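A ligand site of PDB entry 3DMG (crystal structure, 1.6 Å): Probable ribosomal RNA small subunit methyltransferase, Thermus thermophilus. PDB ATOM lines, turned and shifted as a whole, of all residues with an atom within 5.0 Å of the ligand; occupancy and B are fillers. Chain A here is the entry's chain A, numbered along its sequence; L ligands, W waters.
The side-chain hydroxyl (OG) of Ser 216 lies within hydrogen-bond range of an oxygen (O1) of the ligand (2.6 Å). The side-chain carboxylate (OE2) of Glu 262 sits at hydrogen-bond distance from an oxygen (O5) of the ligand (2.6 Å). A nitrogen (N1) of the ligand lies within hydrogen-bond range of the backbone carbonyl oxygen (O) of Gly 241 (2.8 Å). The backbone NH (N) of Val 289 sits at hydrogen-bond distance from a nitrogen (N5) of the ligand (2.9 Å). OD1 of Asp 288 lies within hydrogen-bond range of N4 of the ligand. The backbone NH (N) of Asp 263 lies within hydrogen-bond range of a nitrogen (N6) of the ligand, 3.3 Å away. OH of Tyr 8 is in hydrogen-bond range of N4 of the ligand, at 3.3 Å. The backbone carbonyl oxygen of Ala 242 sits close to a nitrogen (N1) of the ligand (3.4 Å).
The side-chain carboxylate (OE1) of Glu 262 sits at hydrogen-bond distance from the backbone NH (N) of Ala 242, 3.5 Å away. OE1 of Glu 262 lies within hydrogen-bond range of N of Gly 243. The backbone NH of Ser 287 sits at hydrogen-bond distance from the backbone carbonyl oxygen of Glu 262, 2.9 Å away. OE2 of Glu 262 sits at hydrogen-bond distance from N of Asp 264 (3.0 Å). The backbone carbonyl oxygen (O) of Val 289 is in hydrogen-bond range of the side-chain hydroxyl (OG) of Ser 287 (2.7 Å). OH of Tyr 8 is in hydrogen-bond range of OD1 of Asp 288 (2.6 Å). The backbone NH of Asp 263 is in hydrogen-bond range of the backbone carbonyl oxygen of Ser 287. The backbone carbonyl oxygen of Val 261 lies within hydrogen-bond range of the backbone NH of Ala 242 (3.0 Å).
The backbone carbonyl oxygen (O) of Asn 305 lies close to a sulfur (S1) of the ligand (3.6 Å). Phe 207 touches the ligand. Gly 243 touches the ligand. Ala 246 touches the ligand (CB to O2, 3.4 Å). Leu 247 touches the ligand. Ser 287 touches the ligand (O to N5, 3.5 Å). Pro 307 touches the ligand. Val 318 touches the ligand (CG1 to N3, 3.5 Å). Phe 322 touches the ligand (CZ to N6, 3.7 Å). Hydrophobic or aromatic side chains that line the ligand: Phe 207, Ala 246, Leu 247, Val 289, Pro 307, Val 318 and Phe 322. 17 residues have an atom within 4 Å of the ligand: Tyr 8, Phe 207, Ser 216, Gly 241, Ala 242, Gly 243, Ala 246, Leu 247, Glu 262, Asp 263, Ser 287, Asp 288, Val 289, Asn 305, Pro 307, Val 318 and Phe 322.
Water W4 lies within hydrogen-bond range of O2 of the ligand (2.7 Å), N of Ala 246 (3.0 Å) and N of Tyr 244 (3.3 Å). Water W9 lies within hydrogen-bond range of O2 of the ligand (2.8 Å), N of Asp 213 (2.9 Å) and OH of Tyr 244 (3.0 Å). Water W8 lies within hydrogen-bond range of the side-chain carboxylate of Asp 239 (2.8 Å), a nitrogen (N1) of the ligand (2.8 Å), the backbone NH of Asn 305 (3.0 Å) and the backbone carbonyl oxygen of Gly 241 (3.1 Å). Water W6 lies within hydrogen-bond range of OD2 of Asp 239 (2.6 Å), O of Ala 242 (2.7 Å), N1 of the ligand (2.9 Å), N of Leu 247 (2.9 Å) and N of Ala 246 (3.5 Å). Water W11 bridges the side-chain carboxylate (OD2) of Asp 263 (2.9 Å) and a nitrogen (N4) of the ligand (3.0 Å). Water W2 lies within hydrogen-bond range of O of Pro 306 (2.8 Å) and S1 of the ligand (3.3 Å).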
ATOM      1  N   TYR A   8      18.571  37.025 -27.809  1.00  0.00           N
ATOM      2  CA  TYR A   8      17.794  35.830 -28.130  1.00  0.00           C
ATOM      3  C   TYR A   8      17.072  35.973 -29.492  1.00  0.00           C
ATOM      4  O   TYR A   8      17.043  35.041 -30.308  1.00  0.00           O
ATOM      5  CB  TYR A   8      16.765  35.467 -27.024  1.00  0.00           C
ATOM      6  CG  TYR A   8      15.954  34.300 -27.528  1.00  0.00           C
ATOM      7  CD1 TYR A   8      16.458  33.011 -27.486  1.00  0.00           C
ATOM      8  CD2 TYR A   8      14.733  34.501 -28.208  1.00  0.00           C
ATOM      9  CE1 TYR A   8      15.775  31.934 -28.041  1.00  0.00           C
ATOM     10  CE2 TYR A   8      14.044  33.453 -28.783  1.00  0.00           C
ATOM     11  CZ  TYR A   8      14.555  32.167 -28.701  1.00  0.00           C
ATOM     12  OH  TYR A   8      13.890  31.113 -29.295  1.00  0.00           O
ATOM     13  N   PHE A 207       4.587  17.938 -27.725  1.00  0.00           N
ATOM     14  CA  PHE A 207       5.027  17.522 -26.402  1.00  0.00           C
ATOM     15  C   PHE A 207       3.898  16.756 -25.722  1.00  0.00           C
ATOM     16  O   PHE A 207       2.726  17.192 -25.738  1.00  0.00           O
ATOM     17  CB  PHE A 207       5.397  18.751 -25.573  1.00  0.00           C
ATOM     18  CG  PHE A 207       5.741  18.439 -24.138  1.00  0.00           C
ATOM     19  CD1 PHE A 207       6.986  17.936 -23.795  1.00  0.00           C
ATOM     20  CD2 PHE A 207       4.812  18.683 -23.110  1.00  0.00           C
ATOM     21  CE1 PHE A 207       7.309  17.658 -22.452  1.00  0.00           C
ATOM     22  CE2 PHE A 207       5.134  18.415 -21.778  1.00  0.00           C
ATOM     23  CZ  PHE A 207       6.388  17.924 -21.464  1.00  0.00           C
ATOM     24  N   ASP A 213       1.049  15.914 -19.287  1.00  0.00           N
ATOM     25  CA  ASP A 213       2.313  15.744 -18.604  1.00  0.00           C
ATOM     26  C   ASP A 213       2.186  15.972 -17.092  1.00  0.00           C
ATOM     27  O   ASP A 213       1.560  16.917 -16.658  1.00  0.00           O
ATOM     28  CB  ASP A 213       3.400  16.657 -19.179  1.00  0.00           C
ATOM     29  CG  ASP A 213       4.769  16.271 -18.657  1.00  0.00           C
ATOM     30  OD1 ASP A 213       5.265  15.204 -19.049  1.00  0.00           O
ATOM     31  OD2 ASP A 213       5.303  17.013 -17.819  1.00  0.00           O
ATOM     32  N   SER A 216       3.104  19.503 -15.939  1.00  0.00           N
ATOM     33  CA  SER A 216       2.064  20.476 -16.221  1.00  0.00           C
ATOM     34  C   SER A 216       0.928  20.415 -15.196  1.00  0.00           C
ATOM     35  O   SER A 216       0.454  21.448 -14.712  1.00  0.00           O
ATOM     36  CB  SER A 216       1.527  20.281 -17.636  1.00  0.00           C
ATOM     37  OG  SER A 216       2.602  20.258 -18.554  1.00  0.00           O
ATOM     38  N   ASP A 239       1.000  32.044 -21.561  1.00  0.00           N
ATOM     39  CA  ASP A 239       1.439  30.651 -21.422  1.00  0.00           C
ATOM     40  C   ASP A 239       2.604  30.524 -22.393  1.00  0.00           C
ATOM     41  O   ASP A 239       2.400  30.525 -23.633  1.00  0.00           O
ATOM     42  CB  ASP A 239       0.291  29.687 -21.774  1.00  0.00           C
ATOM     43  CG  ASP A 239       0.667  28.226 -21.681  1.00  0.00           C
ATOM     44  OD1 ASP A 239       1.836  27.908 -21.445  1.00  0.00           O
ATOM     45  OD2 ASP A 239      -0.235  27.385 -21.864  1.00  0.00           O
ATOM     46  N   GLY A 241       5.150  28.666 -24.422  1.00  0.00           N
ATOM     47  CA  GLY A 241       5.322  27.306 -24.927  1.00  0.00           C
ATOM     48  C   GLY A 241       4.047  26.513 -24.679  1.00  0.00           C
ATOM     49  O   GLY A 241       4.081  25.515 -23.955  1.00  0.00           O
ATOM     50  N   ALA A 242       2.955  26.973 -25.271  1.00  0.00           N
ATOM     51  CA  ALA A 242       1.605  26.496 -24.881  1.00  0.00           C
ATOM     52  C   ALA A 242       1.316  25.051 -25.301  1.00  0.00           C
ATOM     53  O   ALA A 242       0.444  24.403 -24.712  1.00  0.00           O
ATOM     54  CB  ALA A 242       0.493  27.456 -25.399  1.00  0.00           C
ATOM     55  N   GLY A 243       2.040  24.524 -26.293  1.00  0.00           N
ATOM     56  CA  GLY A 243       1.744  23.170 -26.754  1.00  0.00           C
ATOM     57  C   GLY A 243       0.299  23.017 -27.188  1.00  0.00           C
ATOM     58  O   GLY A 243      -0.295  23.964 -27.705  1.00  0.00           O
ATOM     59  N   TYR A 244      -0.261  21.825 -26.990  1.00  0.00           N
ATOM     60  CA  TYR A 244      -1.687  21.608 -27.341  1.00  0.00           C
ATOM     61  C   TYR A 244      -2.652  22.173 -26.278  1.00  0.00           C
ATOM     62  O   TYR A 244      -3.871  22.061 -26.433  1.00  0.00           O
ATOM     63  CB  TYR A 244      -2.008  20.128 -27.643  1.00  0.00           C
ATOM     64  CG  TYR A 244      -1.723  19.199 -26.498  1.00  0.00           C
ATOM     65  CD1 TYR A 244      -2.526  19.178 -25.357  1.00  0.00           C
ATOM     66  CD2 TYR A 244      -0.644  18.308 -26.575  1.00  0.00           C
ATOM     67  CE1 TYR A 244      -2.256  18.294 -24.304  1.00  0.00           C
ATOM     68  CE2 TYR A 244      -0.353  17.438 -25.551  1.00  0.00           C
ATOM     69  CZ  TYR A 244      -1.154  17.448 -24.410  1.00  0.00           C
ATOM     70  OH  TYR A 244      -0.858  16.591 -23.366  1.00  0.00           O
ATOM     71  N   ALA A 246      -2.260  22.094 -22.415  1.00  0.00           N
ATOM     72  CA  ALA A 246      -2.453  21.470 -21.080  1.00  0.00           C
ATOM     73  C   ALA A 246      -2.601  22.544 -19.998  1.00  0.00           C
ATOM     74  O   ALA A 246      -3.372  22.361 -19.054  1.00  0.00           O
ATOM     75  CB  ALA A 246      -1.308  20.523 -20.760  1.00  0.00           C
ATOM     76  N   LEU A 247      -1.884  23.652 -20.113  1.00  0.00           N
ATOM     77  CA  LEU A 247      -2.073  24.764 -19.155  1.00  0.00           C
ATOM     78  C   LEU A 247      -3.129  25.748 -19.669  1.00  0.00           C
ATOM     79  O   LEU A 247      -3.890  26.322 -18.882  1.00  0.00           O
ATOM     80  CB  LEU A 247      -0.749  25.499 -18.927  1.00  0.00           C
ATOM     81  CG  LEU A 247       0.461  24.673 -18.483  1.00  0.00           C
ATOM     82  CD1 LEU A 247       1.667  25.564 -18.267  1.00  0.00           C
ATOM     83  CD2 LEU A 247       0.151  23.907 -17.206  1.00  0.00           C
ATOM     84  N   VAL A 261       1.732  31.327 -26.512  1.00  0.00           N
ATOM     85  CA  VAL A 261       2.738  31.469 -27.578  1.00  0.00           C
ATOM     86  C   VAL A 261       3.443  30.139 -27.750  1.00  0.00           C
ATOM     87  O   VAL A 261       3.774  29.463 -26.775  1.00  0.00           O
ATOM     88  CB  VAL A 261       3.724  32.629 -27.330  1.00  0.00           C
ATOM     89  CG1 VAL A 261       3.019  33.971 -27.469  1.00  0.00           C
ATOM     90  CG2 VAL A 261       4.476  32.492 -25.966  1.00  0.00           C
ATOM     91  N   GLU A 262       3.621  29.745 -29.006  1.00  0.00           N
ATOM     92  CA  GLU A 262       4.160  28.433 -29.343  1.00  0.00           C
ATOM     93  C   GLU A 262       4.899  28.485 -30.680  1.00  0.00           C
ATOM     94  O   GLU A 262       4.344  28.976 -31.661  1.00  0.00           O
ATOM     95  CB  GLU A 262       2.992  27.453 -29.385  1.00  0.00           C
ATOM     96  CG  GLU A 262       3.310  26.063 -29.959  1.00  0.00           C
ATOM     97  CD  GLU A 262       4.390  25.370 -29.175  1.00  0.00           C
ATOM     98  OE1 GLU A 262       4.214  25.147 -27.943  1.00  0.00           O
ATOM     99  OE2 GLU A 262       5.417  25.015 -29.803  1.00  0.00           O
ATOM    100  N   ASP A 263       6.137  28.002 -30.708  1.00  0.00           N
ATOM    101  CA  ASP A 263       6.969  28.090 -31.897  1.00  0.00           C
ATOM    102  C   ASP A 263       6.600  27.061 -32.950  1.00  0.00           C
ATOM    103  O   ASP A 263       6.917  27.277 -34.121  1.00  0.00           O
ATOM    104  CB  ASP A 263       8.436  27.938 -31.490  1.00  0.00           C
ATOM    105  CG  ASP A 263       9.399  28.202 -32.640  1.00  0.00           C
ATOM    106  OD1 ASP A 263       9.419  29.333 -33.131  1.00  0.00           O
ATOM    107  OD2 ASP A 263      10.147  27.245 -33.024  1.00  0.00           O
ATOM    108  N   ASP A 264       5.974  25.952 -32.547  1.00  0.00           N
ATOM    109  CA  ASP A 264       5.706  24.847 -33.471  1.00  0.00           C
ATOM    110  C   ASP A 264       4.287  24.934 -34.034  1.00  0.00           C
ATOM    111  O   ASP A 264       3.325  24.834 -33.267  1.00  0.00           O
ATOM    112  CB  ASP A 264       5.915  23.498 -32.749  1.00  0.00           C
ATOM    113  CG  ASP A 264       5.375  22.324 -33.533  1.00  0.00           C
ATOM    114  OD1 ASP A 264       5.617  22.255 -34.737  1.00  0.00           O
ATOM    115  OD2 ASP A 264       4.721  21.440 -32.924  1.00  0.00           O
ATOM    116  N   SER A 267       1.757  22.259 -33.034  1.00  0.00           N
ATOM    117  CA  SER A 267       1.254  22.519 -31.682  1.00  0.00           C
ATOM    118  C   SER A 267       0.241  23.661 -31.632  1.00  0.00           C
ATOM    119  O   SER A 267      -0.768  23.560 -30.928  1.00  0.00           O
ATOM    120  CB  SER A 267       2.401  22.751 -30.691  1.00  0.00           C
ATOM    121  OG  SER A 267       3.195  21.571 -30.608  1.00  0.00           O
ATOM    122  N   SER A 287       4.518  31.725 -32.526  1.00  0.00           N
ATOM    123  CA  SER A 287       5.427  32.759 -32.083  1.00  0.00           C
ATOM    124  C   SER A 287       6.709  32.167 -31.545  1.00  0.00           C
ATOM    125  O   SER A 287       6.678  31.152 -30.866  1.00  0.00           O
ATOM    126  CB  SER A 287       4.728  33.532 -30.962  1.00  0.00           C
ATOM    127  OG  SER A 287       5.515  34.641 -30.509  1.00  0.00           O
ATOM    128  N   ASP A 288       7.839  32.811 -31.864  1.00  0.00           N
ATOM    129  CA  ASP A 288       9.118  32.468 -31.248  1.00  0.00           C
ATOM    130  C   ASP A 288       9.196  33.251 -29.945  1.00  0.00           C
ATOM    131  O   ASP A 288       9.424  34.474 -29.949  1.00  0.00           O
ATOM    132  CB  ASP A 288      10.267  32.873 -32.165  1.00  0.00           C
ATOM    133  CG  ASP A 288      11.628  32.547 -31.583  1.00  0.00           C
ATOM    134  OD1 ASP A 288      11.705  31.802 -30.587  1.00  0.00           O
ATOM    135  OD2 ASP A 288      12.622  33.019 -32.161  1.00  0.00           O
ATOM    136  N   VAL A 289       8.969  32.541 -28.843  1.00  0.00           N
ATOM    137  CA  VAL A 289       8.788  33.192 -27.529  1.00  0.00           C
ATOM    138  C   VAL A 289       7.741  34.322 -27.672  1.00  0.00           C
ATOM    139  O   VAL A 289       6.601  34.056 -28.101  1.00  0.00           O
ATOM    140  CB  VAL A 289      10.134  33.596 -26.845  1.00  0.00           C
ATOM    141  CG1 VAL A 289       9.927  33.866 -25.360  1.00  0.00           C
ATOM    142  CG2 VAL A 289      11.181  32.488 -27.033  1.00  0.00           C
ATOM    143  N   ASN A 305       5.797  25.525 -18.684  1.00  0.00           N
ATOM    144  CA  ASN A 305       6.537  24.262 -18.573  1.00  0.00           C
ATOM    145  C   ASN A 305       7.558  24.323 -19.717  1.00  0.00           C
ATOM    146  O   ASN A 305       7.239  23.941 -20.842  1.00  0.00           O
ATOM    147  CB  ASN A 305       5.594  23.063 -18.726  1.00  0.00           C
ATOM    148  CG  ASN A 305       6.308  21.765 -18.568  1.00  0.00           C
ATOM    149  OD1 ASN A 305       7.514  21.742 -18.372  1.00  0.00           O
ATOM    150  ND2 ASN A 305       5.575  20.648 -18.625  1.00  0.00           N
ATOM    151  N   PRO A 306       8.757  24.885 -19.468  1.00  0.00           N
ATOM    152  CA  PRO A 306       9.658  25.145 -20.603  1.00  0.00           C
ATOM    153  C   PRO A 306      10.207  23.889 -21.250  1.00  0.00           C
ATOM    154  O   PRO A 306      10.245  22.816 -20.615  1.00  0.00           O
ATOM    155  CB  PRO A 306      10.811  25.954 -19.979  1.00  0.00           C
ATOM    156  CG  PRO A 306      10.261  26.478 -18.693  1.00  0.00           C
ATOM    157  CD  PRO A 306       9.308  25.418 -18.206  1.00  0.00           C
ATOM    158  N   PRO A 307      10.668  24.002 -22.499  1.00  0.00           N
ATOM    159  CA  PRO A 307      11.315  22.851 -23.130  1.00  0.00           C
ATOM    160  C   PRO A 307      12.569  22.434 -22.365  1.00  0.00           C
ATOM    161  O   PRO A 307      13.168  23.259 -21.674  1.00  0.00           O
ATOM    162  CB  PRO A 307      11.697  23.384 -24.509  1.00  0.00           C
ATOM    163  CG  PRO A 307      11.705  24.848 -24.372  1.00  0.00           C
ATOM    164  CD  PRO A 307      10.673  25.191 -23.373  1.00  0.00           C
ATOM    165  N   VAL A 318      16.182  28.675 -25.280  1.00  0.00           N
ATOM    166  CA  VAL A 318      14.767  29.064 -25.334  1.00  0.00           C
ATOM    167  C   VAL A 318      14.191  29.175 -23.936  1.00  0.00           C
ATOM    168  O   VAL A 318      13.489  30.130 -23.609  1.00  0.00           O
ATOM    169  CB  VAL A 318      13.921  28.064 -26.164  1.00  0.00           C
ATOM    170  CG1 VAL A 318      12.431  28.350 -26.003  1.00  0.00           C
ATOM    171  CG2 VAL A 318      14.318  28.126 -27.638  1.00  0.00           C
ATOM    172  N   PHE A 322      12.564  32.252 -21.907  1.00  0.00           N
ATOM    173  CA  PHE A 322      11.232  32.248 -21.309  1.00  0.00           C
ATOM    174  C   PHE A 322      11.262  33.000 -19.970  1.00  0.00           C
ATOM    175  O   PHE A 322      10.367  33.777 -19.666  1.00  0.00           O
ATOM    176  CB  PHE A 322      10.762  30.822 -21.032  1.00  0.00           C
ATOM    177  CG  PHE A 322      10.136  30.099 -22.218  1.00  0.00           C
ATOM    178  CD1 PHE A 322      10.217  30.575 -23.520  1.00  0.00           C
ATOM    179  CD2 PHE A 322       9.454  28.931 -21.979  1.00  0.00           C
ATOM    180  CE1 PHE A 322       9.609  29.861 -24.564  1.00  0.00           C
ATOM    181  CE2 PHE A 322       8.856  28.210 -22.993  1.00  0.00           C
ATOM    182  CZ  PHE A 322       8.917  28.681 -24.296  1.00  0.00           C
HETATM  183  N1  LIG L   1       2.661  23.983 -22.116  1.00  0.00           N
HETATM  184  C1  LIG L   1       2.546  22.605 -22.724  1.00  0.00           C
HETATM  185  C2  LIG L   1       3.809  22.209 -23.483  1.00  0.00           C
HETATM  186  C3  LIG L   1       5.106  22.306 -22.690  1.00  0.00           C
HETATM  187  S1  LIG L   1       6.544  21.589 -23.543  1.00  0.00           S
HETATM  188  C4  LIG L   1       2.301  21.582 -21.630  1.00  0.00           C
HETATM  189  O1  LIG L   1       2.514  21.962 -20.463  1.00  0.00           O
HETATM  190  O2  LIG L   1       1.930  20.450 -21.939  1.00  0.00           O
HETATM  191  C5  LIG L   1       7.418  23.091 -24.080  1.00  0.00           C
HETATM  192  C6  LIG L   1       6.767  23.759 -25.292  1.00  0.00           C
HETATM  193  O3  LIG L   1       7.627  24.853 -25.605  1.00  0.00           O
HETATM  194  C7  LIG L   1       6.598  22.864 -26.540  1.00  0.00           C
HETATM  195  O4  LIG L   1       5.240  22.866 -26.968  1.00  0.00           O
HETATM  196  C8  LIG L   1       7.551  23.561 -27.525  1.00  0.00           C
HETATM  197  O5  LIG L   1       7.200  23.390 -28.875  1.00  0.00           O
HETATM  198  C9  LIG L   1       7.529  24.977 -26.999  1.00  0.00           C
HETATM  199  N2  LIG L   1       8.619  25.779 -27.542  1.00  0.00           N
HETATM  200  C10 LIG L   1       9.886  25.356 -27.870  1.00  0.00           C
HETATM  201  N3  LIG L   1      10.565  26.435 -28.338  1.00  0.00           N
HETATM  202  C11 LIG L   1       9.751  27.521 -28.292  1.00  0.00           C
HETATM  203  C12 LIG L   1       9.922  28.854 -28.683  1.00  0.00           C
HETATM  204  N4  LIG L   1      11.075  29.301 -29.228  1.00  0.00           N
HETATM  205  N5  LIG L   1       8.845  29.698 -28.485  1.00  0.00           N
HETATM  206  C13 LIG L   1       7.639  29.268 -27.974  1.00  0.00           C
HETATM  207  N6  LIG L   1       7.441  27.938 -27.636  1.00  0.00           N
HETATM  208  C14 LIG L   1       8.513  27.104 -27.794  1.00  0.00           C
HETATM  209  O   HOH W   1      10.994  22.252 -27.603  1.00  0.00           O
HETATM  210  O   HOH W   2       8.894  20.517 -21.502  1.00  0.00           O
HETATM  211  O   HOH W   3       9.208  23.104 -30.831  1.00  0.00           O
HETATM  212  O   HOH W   4      -0.023  20.787 -23.831  1.00  0.00           O
HETATM  213  O   HOH W   5      12.941  25.134 -29.564  1.00  0.00           O
HETATM  214  O   HOH W   6      -0.085  24.805 -22.119  1.00  0.00           O
HETATM  215  O   HOH W   7       3.914  20.760 -28.096  1.00  0.00           O
HETATM  216  O   HOH W   8       4.025  26.180 -20.956  1.00  0.00           O
HETATM  217  O   HOH W   9       0.864  17.931 -21.297  1.00  0.00           O
HETATM  218  O   HOH W  10       6.966  20.521 -29.298  1.00  0.00           O
HETATM  219  O   HOH W  11      12.331  27.312 -31.087  1.00  0.00           O
